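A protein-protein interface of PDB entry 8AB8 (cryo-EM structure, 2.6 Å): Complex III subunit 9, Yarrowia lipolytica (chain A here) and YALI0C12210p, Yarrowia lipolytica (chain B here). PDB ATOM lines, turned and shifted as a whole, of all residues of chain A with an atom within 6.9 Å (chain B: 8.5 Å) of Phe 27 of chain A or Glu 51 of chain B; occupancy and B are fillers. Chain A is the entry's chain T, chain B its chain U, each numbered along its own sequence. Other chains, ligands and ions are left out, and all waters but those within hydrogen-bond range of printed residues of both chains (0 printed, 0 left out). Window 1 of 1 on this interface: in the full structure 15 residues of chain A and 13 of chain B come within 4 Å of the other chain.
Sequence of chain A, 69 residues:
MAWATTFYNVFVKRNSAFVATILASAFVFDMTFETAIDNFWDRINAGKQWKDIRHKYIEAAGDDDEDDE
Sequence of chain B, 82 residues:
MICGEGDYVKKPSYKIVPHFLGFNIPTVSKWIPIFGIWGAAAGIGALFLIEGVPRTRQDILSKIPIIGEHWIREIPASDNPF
The backbone carbonyl oxygen (O) of His 70 of chain B lies within hydrogen-bond range of the guanidinium group (NH1) of Arg 73 of chain B. OE2 of Glu 51 of chain B is in salt-bridge range of NH2 of Arg 57 of chain B, 3.2 Å away. The indole nitrogen (NE1) of Trp 71 of chain B is in hydrogen-bond range of the side-chain carboxylate (OE2) of Glu 51 of chain B.
The side-chain sulfur (SD) of Met 31 of chain A lies close to the side-chain carboxylate (OE2) of Glu 51 of chain B. SD of Met 31 of chain A is in hydrogen-bond range of NE2 of His 70 of chain B, at 3.4 Å.
Ala 26 of chain A touches one residue of chain B. Of the printed residues of chain A, Trp 71 of chain B touches Met 31 (3.7 Å). Of the printed residues of chain B, Asp 30 of chain A touches Phe 48. Of the printed residues of chain B, Ala 24 of chain A touches Ile 44. Printed residues of chain A within 4 Å of Ile 44 of chain B: Leu 23 and Ala 24. Printed residues of chain A within 4 Å of His 70 of chain B: Met 31 (3.4 Å). The nearest residue of chain A that does not touch Glu 51 of chain B is Asp 30 of chain A (4.6 Å). The nearest printed residue of chain B that does not touch Asp 30 of chain A is Glu 51 of chain B (4.6 Å).
Of the 23 printed residues of chain B, 5 touch a printed residue of chain A. Printed residues of chain B that touch a printed residue of chain A: Ile 44, Phe 48, Glu 51, His 70 and Trp 71. Hydrophobic or aromatic side chains of chain B within 4 Å of the printed part of chain A: Ile 44, Phe 48, His 70 and Trp 71. Along chain B the printed residues that touch a printed residue of chain A span positions 44 to 71. Of the 11 printed residues of chain A, 6 touch a printed residue of chain B. Printed residues of chain A that touch a printed residue of chain B: Leu 23, Ala 24, Ala 26, Phe 27, Asp 30 and Met 31. Hydrophobic or aromatic side chains of chain A that line the printed part of chain B: Ala 26, Phe 27 and Met 31. Among the printed residues, no Asp or Glu carboxylate lies within 4 Å of a Lys or Arg side-chain nitrogen of the other chain.
CG2 of Ile 44 of chain B touches C of Leu 23 of chain A, 3.9 Å away. Ile 44 of chain B touches Ala 24 of chain A (CG2 to N, 3.8 Å). Ala 26 of chain A touches Phe 48 of chain B. CE2 of Phe 27 of chain A touches CA of Phe 48 of chain B (3.5 Å). Phe 27 of chain A touches Glu 51 of chain B (CE1 to CG, 3.9 Å). CB of Asp 30 of chain A touches CE1 of Phe 48 of chain B, 3.7 Å away. Trp 71 of chain B touches Met 31 of chain A (CZ2 to SD, 3.7 Å).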
ATOM      1  N   ILE A  22      -7.644 -37.171   8.042  1.00  0.00           N
ATOM      2  CA  ILE A  22      -8.215 -37.951   9.135  1.00  0.00           C
ATOM      3  C   ILE A  22      -9.073 -37.025  10.004  1.00  0.00           C
ATOM      4  O   ILE A  22     -10.199 -37.378  10.332  1.00  0.00           O
ATOM      5  CB  ILE A  22      -7.123 -38.717   9.927  1.00  0.00           C
ATOM      6  CG1 ILE A  22      -6.558 -39.909   9.146  1.00  0.00           C
ATOM      7  CG2 ILE A  22      -7.595 -39.134  11.317  1.00  0.00           C
ATOM      8  CD1 ILE A  22      -5.165 -40.356   9.599  1.00  0.00           C
ATOM      9  N   LEU A  23      -8.554 -35.838  10.342  1.00  0.00           N
ATOM     10  CA  LEU A  23      -9.271 -34.911  11.206  1.00  0.00           C
ATOM     11  C   LEU A  23     -10.515 -34.361  10.517  1.00  0.00           C
ATOM     12  O   LEU A  23     -11.544 -34.227  11.172  1.00  0.00           O
ATOM     13  CB  LEU A  23      -8.354 -33.786  11.685  1.00  0.00           C
ATOM     14  CG  LEU A  23      -7.218 -34.247  12.589  1.00  0.00           C
ATOM     15  CD1 LEU A  23      -6.332 -33.079  12.979  1.00  0.00           C
ATOM     16  CD2 LEU A  23      -7.759 -34.965  13.818  1.00  0.00           C
ATOM     17  N   ALA A  24     -10.425 -34.066   9.213  1.00  0.00           N
ATOM     18  CA  ALA A  24     -11.587 -33.583   8.477  1.00  0.00           C
ATOM     19  C   ALA A  24     -12.665 -34.664   8.422  1.00  0.00           C
ATOM     20  O   ALA A  24     -13.844 -34.365   8.581  1.00  0.00           O
ATOM     21  CB  ALA A  24     -11.197 -33.111   7.100  1.00  0.00           C
ATOM     22  N   SER A  25     -12.243 -35.917   8.229  1.00  0.00           N
ATOM     23  CA  SER A  25     -13.147 -37.057   8.224  1.00  0.00           C
ATOM     24  C   SER A  25     -13.800 -37.240   9.590  1.00  0.00           C
ATOM     25  O   SER A  25     -14.970 -37.605   9.664  1.00  0.00           O
ATOM     26  CB  SER A  25     -12.421 -38.305   7.819  1.00  0.00           C
ATOM     27  OG  SER A  25     -11.776 -38.098   6.575  1.00  0.00           O
ATOM     28  N   ALA A  26     -13.024 -37.014  10.657  1.00  0.00           N
ATOM     29  CA  ALA A  26     -13.532 -37.164  12.012  1.00  0.00           C
ATOM     30  C   ALA A  26     -14.624 -36.130  12.258  1.00  0.00           C
ATOM     31  O   ALA A  26     -15.624 -36.447  12.893  1.00  0.00           O
ATOM     32  CB  ALA A  26     -12.419 -37.076  13.030  1.00  0.00           C
ATOM     33  N   PHE A  27     -14.428 -34.917  11.722  1.00  0.00           N
ATOM     34  CA  PHE A  27     -15.377 -33.824  11.859  1.00  0.00           C
ATOM     35  C   PHE A  27     -16.676 -34.195  11.149  1.00  0.00           C
ATOM     36  O   PHE A  27     -17.750 -34.088  11.736  1.00  0.00           O
ATOM     37  CB  PHE A  27     -14.766 -32.514  11.348  1.00  0.00           C
ATOM     38  CG  PHE A  27     -15.284 -31.238  11.968  1.00  0.00           C
ATOM     39  CD1 PHE A  27     -16.625 -31.080  12.306  1.00  0.00           C
ATOM     40  CD2 PHE A  27     -14.427 -30.164  12.177  1.00  0.00           C
ATOM     41  CE1 PHE A  27     -17.089 -29.899  12.869  1.00  0.00           C
ATOM     42  CE2 PHE A  27     -14.891 -28.978  12.732  1.00  0.00           C
ATOM     43  CZ  PHE A  27     -16.221 -28.847  13.079  1.00  0.00           C
ATOM     44  N   VAL A  28     -16.561 -34.700   9.917  1.00  0.00           N
ATOM     45  CA  VAL A  28     -17.732 -35.090   9.145  1.00  0.00           C
ATOM     46  C   VAL A  28     -18.445 -36.257   9.822  1.00  0.00           C
ATOM     47  O   VAL A  28     -19.665 -36.220   9.968  1.00  0.00           O
ATOM     48  CB  VAL A  28     -17.378 -35.423   7.687  1.00  0.00           C
ATOM     49  CG1 VAL A  28     -18.584 -35.941   6.924  1.00  0.00           C
ATOM     50  CG2 VAL A  28     -16.770 -34.222   6.985  1.00  0.00           C
ATOM     51  N   PHE A  29     -17.685 -37.280  10.228  1.00  0.00           N
ATOM     52  CA  PHE A  29     -18.256 -38.440  10.892  1.00  0.00           C
ATOM     53  C   PHE A  29     -19.053 -37.997  12.114  1.00  0.00           C
ATOM     54  O   PHE A  29     -20.216 -38.360  12.255  1.00  0.00           O
ATOM     55  CB  PHE A  29     -17.182 -39.453  11.291  1.00  0.00           C
ATOM     56  CG  PHE A  29     -17.702 -40.530  12.209  1.00  0.00           C
ATOM     57  CD1 PHE A  29     -18.332 -41.655  11.691  1.00  0.00           C
ATOM     58  CD2 PHE A  29     -17.599 -40.406  13.593  1.00  0.00           C
ATOM     59  CE1 PHE A  29     -18.825 -42.644  12.533  1.00  0.00           C
ATOM     60  CE2 PHE A  29     -18.100 -41.392  14.437  1.00  0.00           C
ATOM     61  CZ  PHE A  29     -18.719 -42.506  13.904  1.00  0.00           C
ATOM     62  N   ASP A  30     -18.424 -37.186  12.970  1.00  0.00           N
ATOM     63  CA  ASP A  30     -19.030 -36.702  14.199  1.00  0.00           C
ATOM     64  C   ASP A  30     -20.390 -36.056  13.937  1.00  0.00           C
ATOM     65  O   ASP A  30     -21.338 -36.323  14.671  1.00  0.00           O
ATOM     66  CB  ASP A  30     -18.098 -35.739  14.927  1.00  0.00           C
ATOM     67  CG  ASP A  30     -18.365 -35.666  16.420  1.00  0.00           C
ATOM     68  OD1 ASP A  30     -18.012 -36.640  17.126  1.00  0.00           O
ATOM     69  OD2 ASP A  30     -18.915 -34.640  16.876  1.00  0.00           O
ATOM     70  N   MET A  31     -20.485 -35.217  12.899  1.00  0.00           N
ATOM     71  CA  MET A  31     -21.704 -34.471  12.626  1.00  0.00           C
ATOM     72  C   MET A  31     -22.787 -35.375  12.041  1.00  0.00           C
ATOM     73  O   MET A  31     -23.953 -35.266  12.420  1.00  0.00           O
ATOM     74  CB  MET A  31     -21.440 -33.287  11.693  1.00  0.00           C
ATOM     75  CG  MET A  31     -20.455 -32.289  12.276  1.00  0.00           C
ATOM     76  SD  MET A  31     -20.953 -31.519  13.850  1.00  0.00           S
ATOM     77  CE  MET A  31     -20.007 -32.468  15.041  1.00  0.00           C
ATOM     78  N   THR A  32     -22.388 -36.279  11.149  1.00  0.00           N
ATOM     79  CA  THR A  32     -23.346 -37.125  10.465  1.00  0.00           C
ATOM     80  C   THR A  32     -23.824 -38.236  11.391  1.00  0.00           C
ATOM     81  O   THR A  32     -25.004 -38.562  11.388  1.00  0.00           O
ATOM     82  CB  THR A  32     -22.766 -37.653   9.153  1.00  0.00           C
ATOM     83  OG1 THR A  32     -21.529 -38.259   9.518  1.00  0.00           O
ATOM     84  CG2 THR A  32     -22.503 -36.541   8.162  1.00  0.00           C
ATOM     85  N   GLY B  43      -5.805 -26.222  12.260  1.00  0.00           N
ATOM     86  CA  GLY B  43      -7.028 -25.442  12.145  1.00  0.00           C
ATOM     87  C   GLY B  43      -8.267 -26.323  12.250  1.00  0.00           C
ATOM     88  O   GLY B  43      -9.133 -26.063  13.078  1.00  0.00           O
ATOM     89  N   ILE B  44      -8.331 -27.369  11.415  1.00  0.00           N
ATOM     90  CA  ILE B  44      -9.445 -28.304  11.443  1.00  0.00           C
ATOM     91  C   ILE B  44      -9.548 -28.891  12.848  1.00  0.00           C
ATOM     92  O   ILE B  44     -10.640 -28.964  13.398  1.00  0.00           O
ATOM     93  CB  ILE B  44      -9.300 -29.419  10.387  1.00  0.00           C
ATOM     94  CG1 ILE B  44      -9.286 -28.880   8.954  1.00  0.00           C
ATOM     95  CG2 ILE B  44     -10.367 -30.488  10.576  1.00  0.00           C
ATOM     96  CD1 ILE B  44      -8.584 -29.789   7.955  1.00  0.00           C
ATOM     97  N   GLY B  45      -8.407 -29.314  13.403  1.00  0.00           N
ATOM     98  CA  GLY B  45      -8.378 -29.967  14.701  1.00  0.00           C
ATOM     99  C   GLY B  45      -8.891 -29.048  15.808  1.00  0.00           C
ATOM    100  O   GLY B  45      -9.692 -29.467  16.643  1.00  0.00           O
ATOM    101  N   ALA B  46      -8.424 -27.793  15.783  1.00  0.00           N
ATOM    102  CA  ALA B  46      -8.764 -26.817  16.808  1.00  0.00           C
ATOM    103  C   ALA B  46     -10.260 -26.531  16.746  1.00  0.00           C
ATOM    104  O   ALA B  46     -10.956 -26.591  17.761  1.00  0.00           O
ATOM    105  CB  ALA B  46      -7.950 -25.560  16.631  1.00  0.00           C
ATOM    106  N   LEU B  47     -10.741 -26.289  15.525  1.00  0.00           N
ATOM    107  CA  LEU B  47     -12.133 -25.946  15.310  1.00  0.00           C
ATOM    108  C   LEU B  47     -13.030 -27.103  15.740  1.00  0.00           C
ATOM    109  O   LEU B  47     -14.085 -26.879  16.330  1.00  0.00           O
ATOM    110  CB  LEU B  47     -12.338 -25.583  13.836  1.00  0.00           C
ATOM    111  CG  LEU B  47     -13.748 -25.129  13.463  1.00  0.00           C
ATOM    112  CD1 LEU B  47     -14.112 -23.831  14.171  1.00  0.00           C
ATOM    113  CD2 LEU B  47     -13.866 -24.961  11.956  1.00  0.00           C
ATOM    114  N   PHE B  48     -12.589 -28.326  15.436  1.00  0.00           N
ATOM    115  CA  PHE B  48     -13.287 -29.539  15.815  1.00  0.00           C
ATOM    116  C   PHE B  48     -13.380 -29.661  17.334  1.00  0.00           C
ATOM    117  O   PHE B  48     -14.414 -30.080  17.842  1.00  0.00           O
ATOM    118  CB  PHE B  48     -12.592 -30.746  15.185  1.00  0.00           C
ATOM    119  CG  PHE B  48     -13.243 -32.081  15.434  1.00  0.00           C
ATOM    120  CD1 PHE B  48     -14.623 -32.244  15.336  1.00  0.00           C
ATOM    121  CD2 PHE B  48     -12.464 -33.196  15.722  1.00  0.00           C
ATOM    122  CE1 PHE B  48     -15.211 -33.487  15.548  1.00  0.00           C
ATOM    123  CE2 PHE B  48     -13.051 -34.439  15.922  1.00  0.00           C
ATOM    124  CZ  PHE B  48     -14.422 -34.582  15.836  1.00  0.00           C
ATOM    125  N   LEU B  49     -12.302 -29.298  18.038  1.00  0.00           N
ATOM    126  CA  LEU B  49     -12.268 -29.366  19.491  1.00  0.00           C
ATOM    127  C   LEU B  49     -13.274 -28.413  20.130  1.00  0.00           C
ATOM    128  O   LEU B  49     -13.773 -28.687  21.222  1.00  0.00           O
ATOM    129  CB  LEU B  49     -10.854 -29.063  19.992  1.00  0.00           C
ATOM    130  CG  LEU B  49      -9.932 -30.272  20.137  1.00  0.00           C
ATOM    131  CD1 LEU B  49      -8.514 -29.831  20.463  1.00  0.00           C
ATOM    132  CD2 LEU B  49     -10.443 -31.221  21.209  1.00  0.00           C
ATOM    133  N   ILE B  50     -13.558 -27.286  19.474  1.00  0.00           N
ATOM    134  CA  ILE B  50     -14.392 -26.286  20.122  1.00  0.00           C
ATOM    135  C   ILE B  50     -15.740 -26.198  19.423  1.00  0.00           C
ATOM    136  O   ILE B  50     -16.459 -25.219  19.595  1.00  0.00           O
ATOM    137  CB  ILE B  50     -13.693 -24.916  20.214  1.00  0.00           C
ATOM    138  CG1 ILE B  50     -13.329 -24.365  18.830  1.00  0.00           C
ATOM    139  CG2 ILE B  50     -12.504 -24.991  21.163  1.00  0.00           C
ATOM    140  CD1 ILE B  50     -13.108 -22.867  18.786  1.00  0.00           C
ATOM    141  N   GLU B  51     -16.062 -27.217  18.627  1.00  0.00           N
ATOM    142  CA  GLU B  51     -17.312 -27.247  17.886  1.00  0.00           C
ATOM    143  C   GLU B  51     -18.505 -27.167  18.845  1.00  0.00           C
ATOM    144  O   GLU B  51     -19.557 -26.640  18.484  1.00  0.00           O
ATOM    145  CB  GLU B  51     -17.336 -28.511  17.025  1.00  0.00           C
ATOM    146  CG  GLU B  51     -18.658 -28.776  16.308  1.00  0.00           C
ATOM    147  CD  GLU B  51     -19.800 -29.429  17.085  1.00  0.00           C
ATOM    148  OE1 GLU B  51     -19.520 -30.245  17.994  1.00  0.00           O
ATOM    149  OE2 GLU B  51     -20.979 -29.139  16.767  1.00  0.00           O
ATOM    150  N   GLY B  52     -18.344 -27.721  20.052  1.00  0.00           N
ATOM    151  CA  GLY B  52     -19.401 -27.740  21.051  1.00  0.00           C
ATOM    152  C   GLY B  52     -19.638 -26.374  21.697  1.00  0.00           C
ATOM    153  O   GLY B  52     -20.751 -26.079  22.127  1.00  0.00           O
ATOM    154  N   VAL B  53     -18.596 -25.541  21.757  1.00  0.00           N
ATOM    155  CA  VAL B  53     -18.717 -24.211  22.335  1.00  0.00           C
ATOM    156  C   VAL B  53     -19.764 -23.423  21.553  1.00  0.00           C
ATOM    157  O   VAL B  53     -19.674 -23.302  20.336  1.00  0.00           O
ATOM    158  CB  VAL B  53     -17.366 -23.480  22.363  1.00  0.00           C
ATOM    159  CG1 VAL B  53     -17.498 -22.079  22.941  1.00  0.00           C
ATOM    160  CG2 VAL B  53     -16.312 -24.285  23.110  1.00  0.00           C
ATOM    161  N   PRO B  54     -20.815 -22.902  22.225  1.00  0.00           N
ATOM    162  CA  PRO B  54     -21.894 -22.179  21.548  1.00  0.00           C
ATOM    163  C   PRO B  54     -21.463 -20.980  20.705  1.00  0.00           C
ATOM    164  O   PRO B  54     -22.074 -20.709  19.676  1.00  0.00           O
ATOM    165  CB  PRO B  54     -22.784 -21.715  22.704  1.00  0.00           C
ATOM    166  CG  PRO B  54     -22.542 -22.752  23.766  1.00  0.00           C
ATOM    167  CD  PRO B  54     -21.064 -23.058  23.666  1.00  0.00           C
ATOM    168  N   ARG B  55     -20.405 -20.288  21.137  1.00  0.00           N
ATOM    169  CA  ARG B  55     -19.885 -19.141  20.412  1.00  0.00           C
ATOM    170  C   ARG B  55     -19.311 -19.565  19.057  1.00  0.00           C
ATOM    171  O   ARG B  55     -19.485 -18.859  18.066  1.00  0.00           O
ATOM    172  CB  ARG B  55     -18.872 -18.388  21.276  1.00  0.00           C
ATOM    173  CG  ARG B  55     -18.418 -17.082  20.645  1.00  0.00           C
ATOM    174  CD  ARG B  55     -17.913 -15.989  21.571  1.00  0.00           C
ATOM    175  NE  ARG B  55     -18.604 -15.845  22.850  1.00  0.00           N
ATOM    176  CZ  ARG B  55     -19.324 -14.798  23.245  1.00  0.00           C
ATOM    177  NH1 ARG B  55     -19.465 -13.736  22.469  1.00  0.00           N
ATOM    178  NH2 ARG B  55     -19.890 -14.813  24.439  1.00  0.00           N
ATOM    179  N   THR B  56     -18.624 -20.712  19.030  1.00  0.00           N
ATOM    180  CA  THR B  56     -18.091 -21.295  17.808  1.00  0.00           C
ATOM    181  C   THR B  56     -19.216 -21.540  16.810  1.00  0.00           C
ATOM    182  O   THR B  56     -19.041 -21.291  15.621  1.00  0.00           O
ATOM    183  CB  THR B  56     -17.418 -22.643  18.078  1.00  0.00           C
ATOM    184  OG1 THR B  56     -16.521 -22.450  19.169  1.00  0.00           O
ATOM    185  CG2 THR B  56     -16.691 -23.220  16.882  1.00  0.00           C
ATOM    186  N   ARG B  57     -20.363 -22.029  17.303  1.00  0.00           N
ATOM    187  CA  ARG B  57     -21.478 -22.343  16.426  1.00  0.00           C
ATOM    188  C   ARG B  57     -22.091 -21.050  15.913  1.00  0.00           C
ATOM    189  O   ARG B  57     -22.286 -20.905  14.713  1.00  0.00           O
ATOM    190  CB  ARG B  57     -22.531 -23.201  17.129  1.00  0.00           C
ATOM    191  CG  ARG B  57     -22.036 -24.596  17.459  1.00  0.00           C
ATOM    192  CD  ARG B  57     -22.909 -25.197  18.530  1.00  0.00           C
ATOM    193  NE  ARG B  57     -22.394 -26.520  18.823  1.00  0.00           N
ATOM    194  CZ  ARG B  57     -23.122 -27.504  19.324  1.00  0.00           C
ATOM    195  NH1 ARG B  57     -24.407 -27.311  19.566  1.00  0.00           N
ATOM    196  NH2 ARG B  57     -22.576 -28.684  19.544  1.00  0.00           N
ATOM    197  N   GLN B  58     -22.319 -20.115  16.843  1.00  0.00           N
ATOM    198  CA  GLN B  58     -22.953 -18.836  16.577  1.00  0.00           C
ATOM    199  C   GLN B  58     -22.132 -18.017  15.577  1.00  0.00           C
ATOM    200  O   GLN B  58     -22.698 -17.503  14.618  1.00  0.00           O
ATOM    201  CB  GLN B  58     -23.246 -18.126  17.901  1.00  0.00           C
ATOM    202  CG  GLN B  58     -24.012 -16.821  17.755  1.00  0.00           C
ATOM    203  CD  GLN B  58     -25.395 -17.029  17.187  1.00  0.00           C
ATOM    204  OE1 GLN B  58     -26.243 -17.689  17.785  1.00  0.00           O
ATOM    205  NE2 GLN B  58     -25.624 -16.469  16.011  1.00  0.00           N
ATOM    206  N   ILE B  60     -19.008 -18.962  13.832  1.00  0.00           N
ATOM    207  CA  ILE B  60     -18.251 -19.584  12.753  1.00  0.00           C
ATOM    208  C   ILE B  60     -19.140 -20.570  11.996  1.00  0.00           C
ATOM    209  O   ILE B  60     -19.404 -20.402  10.808  1.00  0.00           O
ATOM    210  CB  ILE B  60     -16.970 -20.291  13.259  1.00  0.00           C
ATOM    211  CG1 ILE B  60     -16.019 -19.425  14.096  1.00  0.00           C
ATOM    212  CG2 ILE B  60     -16.260 -21.008  12.113  1.00  0.00           C
ATOM    213  CD1 ILE B  60     -15.690 -18.066  13.508  1.00  0.00           C
ATOM    214  N   LEU B  61     -19.566 -21.625  12.697  1.00  0.00           N
ATOM    215  CA  LEU B  61     -20.048 -22.826  12.037  1.00  0.00           C
ATOM    216  C   LEU B  61     -21.403 -22.602  11.370  1.00  0.00           C
ATOM    217  O   LEU B  61     -21.666 -23.203  10.334  1.00  0.00           O
ATOM    218  CB  LEU B  61     -20.104 -23.977  13.045  1.00  0.00           C
ATOM    219  CG  LEU B  61     -18.750 -24.495  13.530  1.00  0.00           C
ATOM    220  CD1 LEU B  61     -18.931 -25.589  14.566  1.00  0.00           C
ATOM    221  CD2 LEU B  61     -17.913 -25.010  12.368  1.00  0.00           C
ATOM    222  N   ILE B  64     -21.343 -21.000   7.660  1.00  0.00           N
ATOM    223  CA  ILE B  64     -20.927 -21.789   6.508  1.00  0.00           C
ATOM    224  C   ILE B  64     -22.151 -22.049   5.629  1.00  0.00           C
ATOM    225  O   ILE B  64     -23.186 -22.485   6.130  1.00  0.00           O
ATOM    226  CB  ILE B  64     -20.223 -23.094   6.944  1.00  0.00           C
ATOM    227  CG1 ILE B  64     -19.003 -22.814   7.830  1.00  0.00           C
ATOM    228  CG2 ILE B  64     -19.868 -23.970   5.746  1.00  0.00           C
ATOM    229  CD1 ILE B  64     -18.517 -24.004   8.644  1.00  0.00           C
ATOM    230  N   ILE B  67     -24.296 -26.100   4.741  1.00  0.00           N
ATOM    231  CA  ILE B  67     -23.900 -26.940   5.860  1.00  0.00           C
ATOM    232  C   ILE B  67     -24.285 -26.272   7.188  1.00  0.00           C
ATOM    233  O   ILE B  67     -24.635 -26.947   8.160  1.00  0.00           O
ATOM    234  CB  ILE B  67     -22.386 -27.208   5.671  1.00  0.00           C
ATOM    235  CG1 ILE B  67     -22.135 -27.986   4.374  1.00  0.00           C
ATOM    236  CG2 ILE B  67     -21.738 -27.912   6.855  1.00  0.00           C
ATOM    237  CD1 ILE B  67     -20.769 -27.759   3.752  1.00  0.00           C
ATOM    238  N   HIS B  70     -26.890 -26.973  10.125  1.00  0.00           N
ATOM    239  CA  HIS B  70     -26.681 -28.056  11.067  1.00  0.00           C
ATOM    240  C   HIS B  70     -26.552 -27.519  12.491  1.00  0.00           C
ATOM    241  O   HIS B  70     -26.845 -28.238  13.442  1.00  0.00           O
ATOM    242  CB  HIS B  70     -25.463 -28.892  10.655  1.00  0.00           C
ATOM    243  CG  HIS B  70     -25.118 -29.960  11.636  1.00  0.00           C
ATOM    244  ND1 HIS B  70     -25.800 -31.159  11.689  1.00  0.00           N
ATOM    245  CD2 HIS B  70     -24.188 -30.007  12.614  1.00  0.00           C
ATOM    246  CE1 HIS B  70     -25.296 -31.903  12.653  1.00  0.00           C
ATOM    247  NE2 HIS B  70     -24.307 -31.216  13.237  1.00  0.00           N
ATOM    248  N   TRP B  71     -26.111 -26.263  12.626  1.00  0.00           N
ATOM    249  CA  TRP B  71     -25.773 -25.713  13.930  1.00  0.00           C
ATOM    250  C   TRP B  71     -26.812 -24.697  14.399  1.00  0.00           C
ATOM    251  O   TRP B  71     -26.652 -24.100  15.462  1.00  0.00           O
ATOM    252  CB  TRP B  71     -24.349 -25.144  13.930  1.00  0.00           C
ATOM    253  CG  TRP B  71     -23.297 -26.207  13.840  1.00  0.00           C
ATOM    254  CD1 TRP B  71     -22.838 -27.004  14.848  1.00  0.00           C
ATOM    255  CD2 TRP B  71     -22.590 -26.616  12.658  1.00  0.00           C
ATOM    256  NE1 TRP B  71     -21.889 -27.870  14.381  1.00  0.00           N
ATOM    257  CE2 TRP B  71     -21.715 -27.659  13.041  1.00  0.00           C
ATOM    258  CE3 TRP B  71     -22.609 -26.200  11.321  1.00  0.00           C
ATOM    259  CZ2 TRP B  71     -20.861 -28.283  12.133  1.00  0.00           C
ATOM    260  CZ3 TRP B  71     -21.764 -26.817  10.424  1.00  0.00           C
ATOM    261  CH2 TRP B  71     -20.904 -27.843  10.828  1.00  0.00           C
ATOM    262  N   ARG B  73     -30.089 -24.725  15.813  1.00  0.00           N
ATOM    263  CA  ARG B  73     -31.076 -25.575  16.459  1.00  0.00           C
ATOM    264  C   ARG B  73     -31.595 -24.863  17.704  1.00  0.00           C
ATOM    265  O   ARG B  73     -30.806 -24.416  18.537  1.00  0.00           O
ATOM    266  CB  ARG B  73     -30.500 -26.966  16.758  1.00  0.00           C
ATOM    267  CG  ARG B  73     -28.998 -27.003  17.008  1.00  0.00           C
ATOM    268  CD  ARG B  73     -28.517 -28.249  17.724  1.00  0.00           C
ATOM    269  NE  ARG B  73     -27.073 -28.417  17.589  1.00  0.00           N
ATOM    270  CZ  ARG B  73     -26.473 -29.325  16.819  1.00  0.00           C
ATOM    271  NH1 ARG B  73     -27.189 -30.181  16.110  1.00  0.00           N
ATOM    272  NH2 ARG B  73     -25.153 -29.378  16.770  1.00  0.00           N
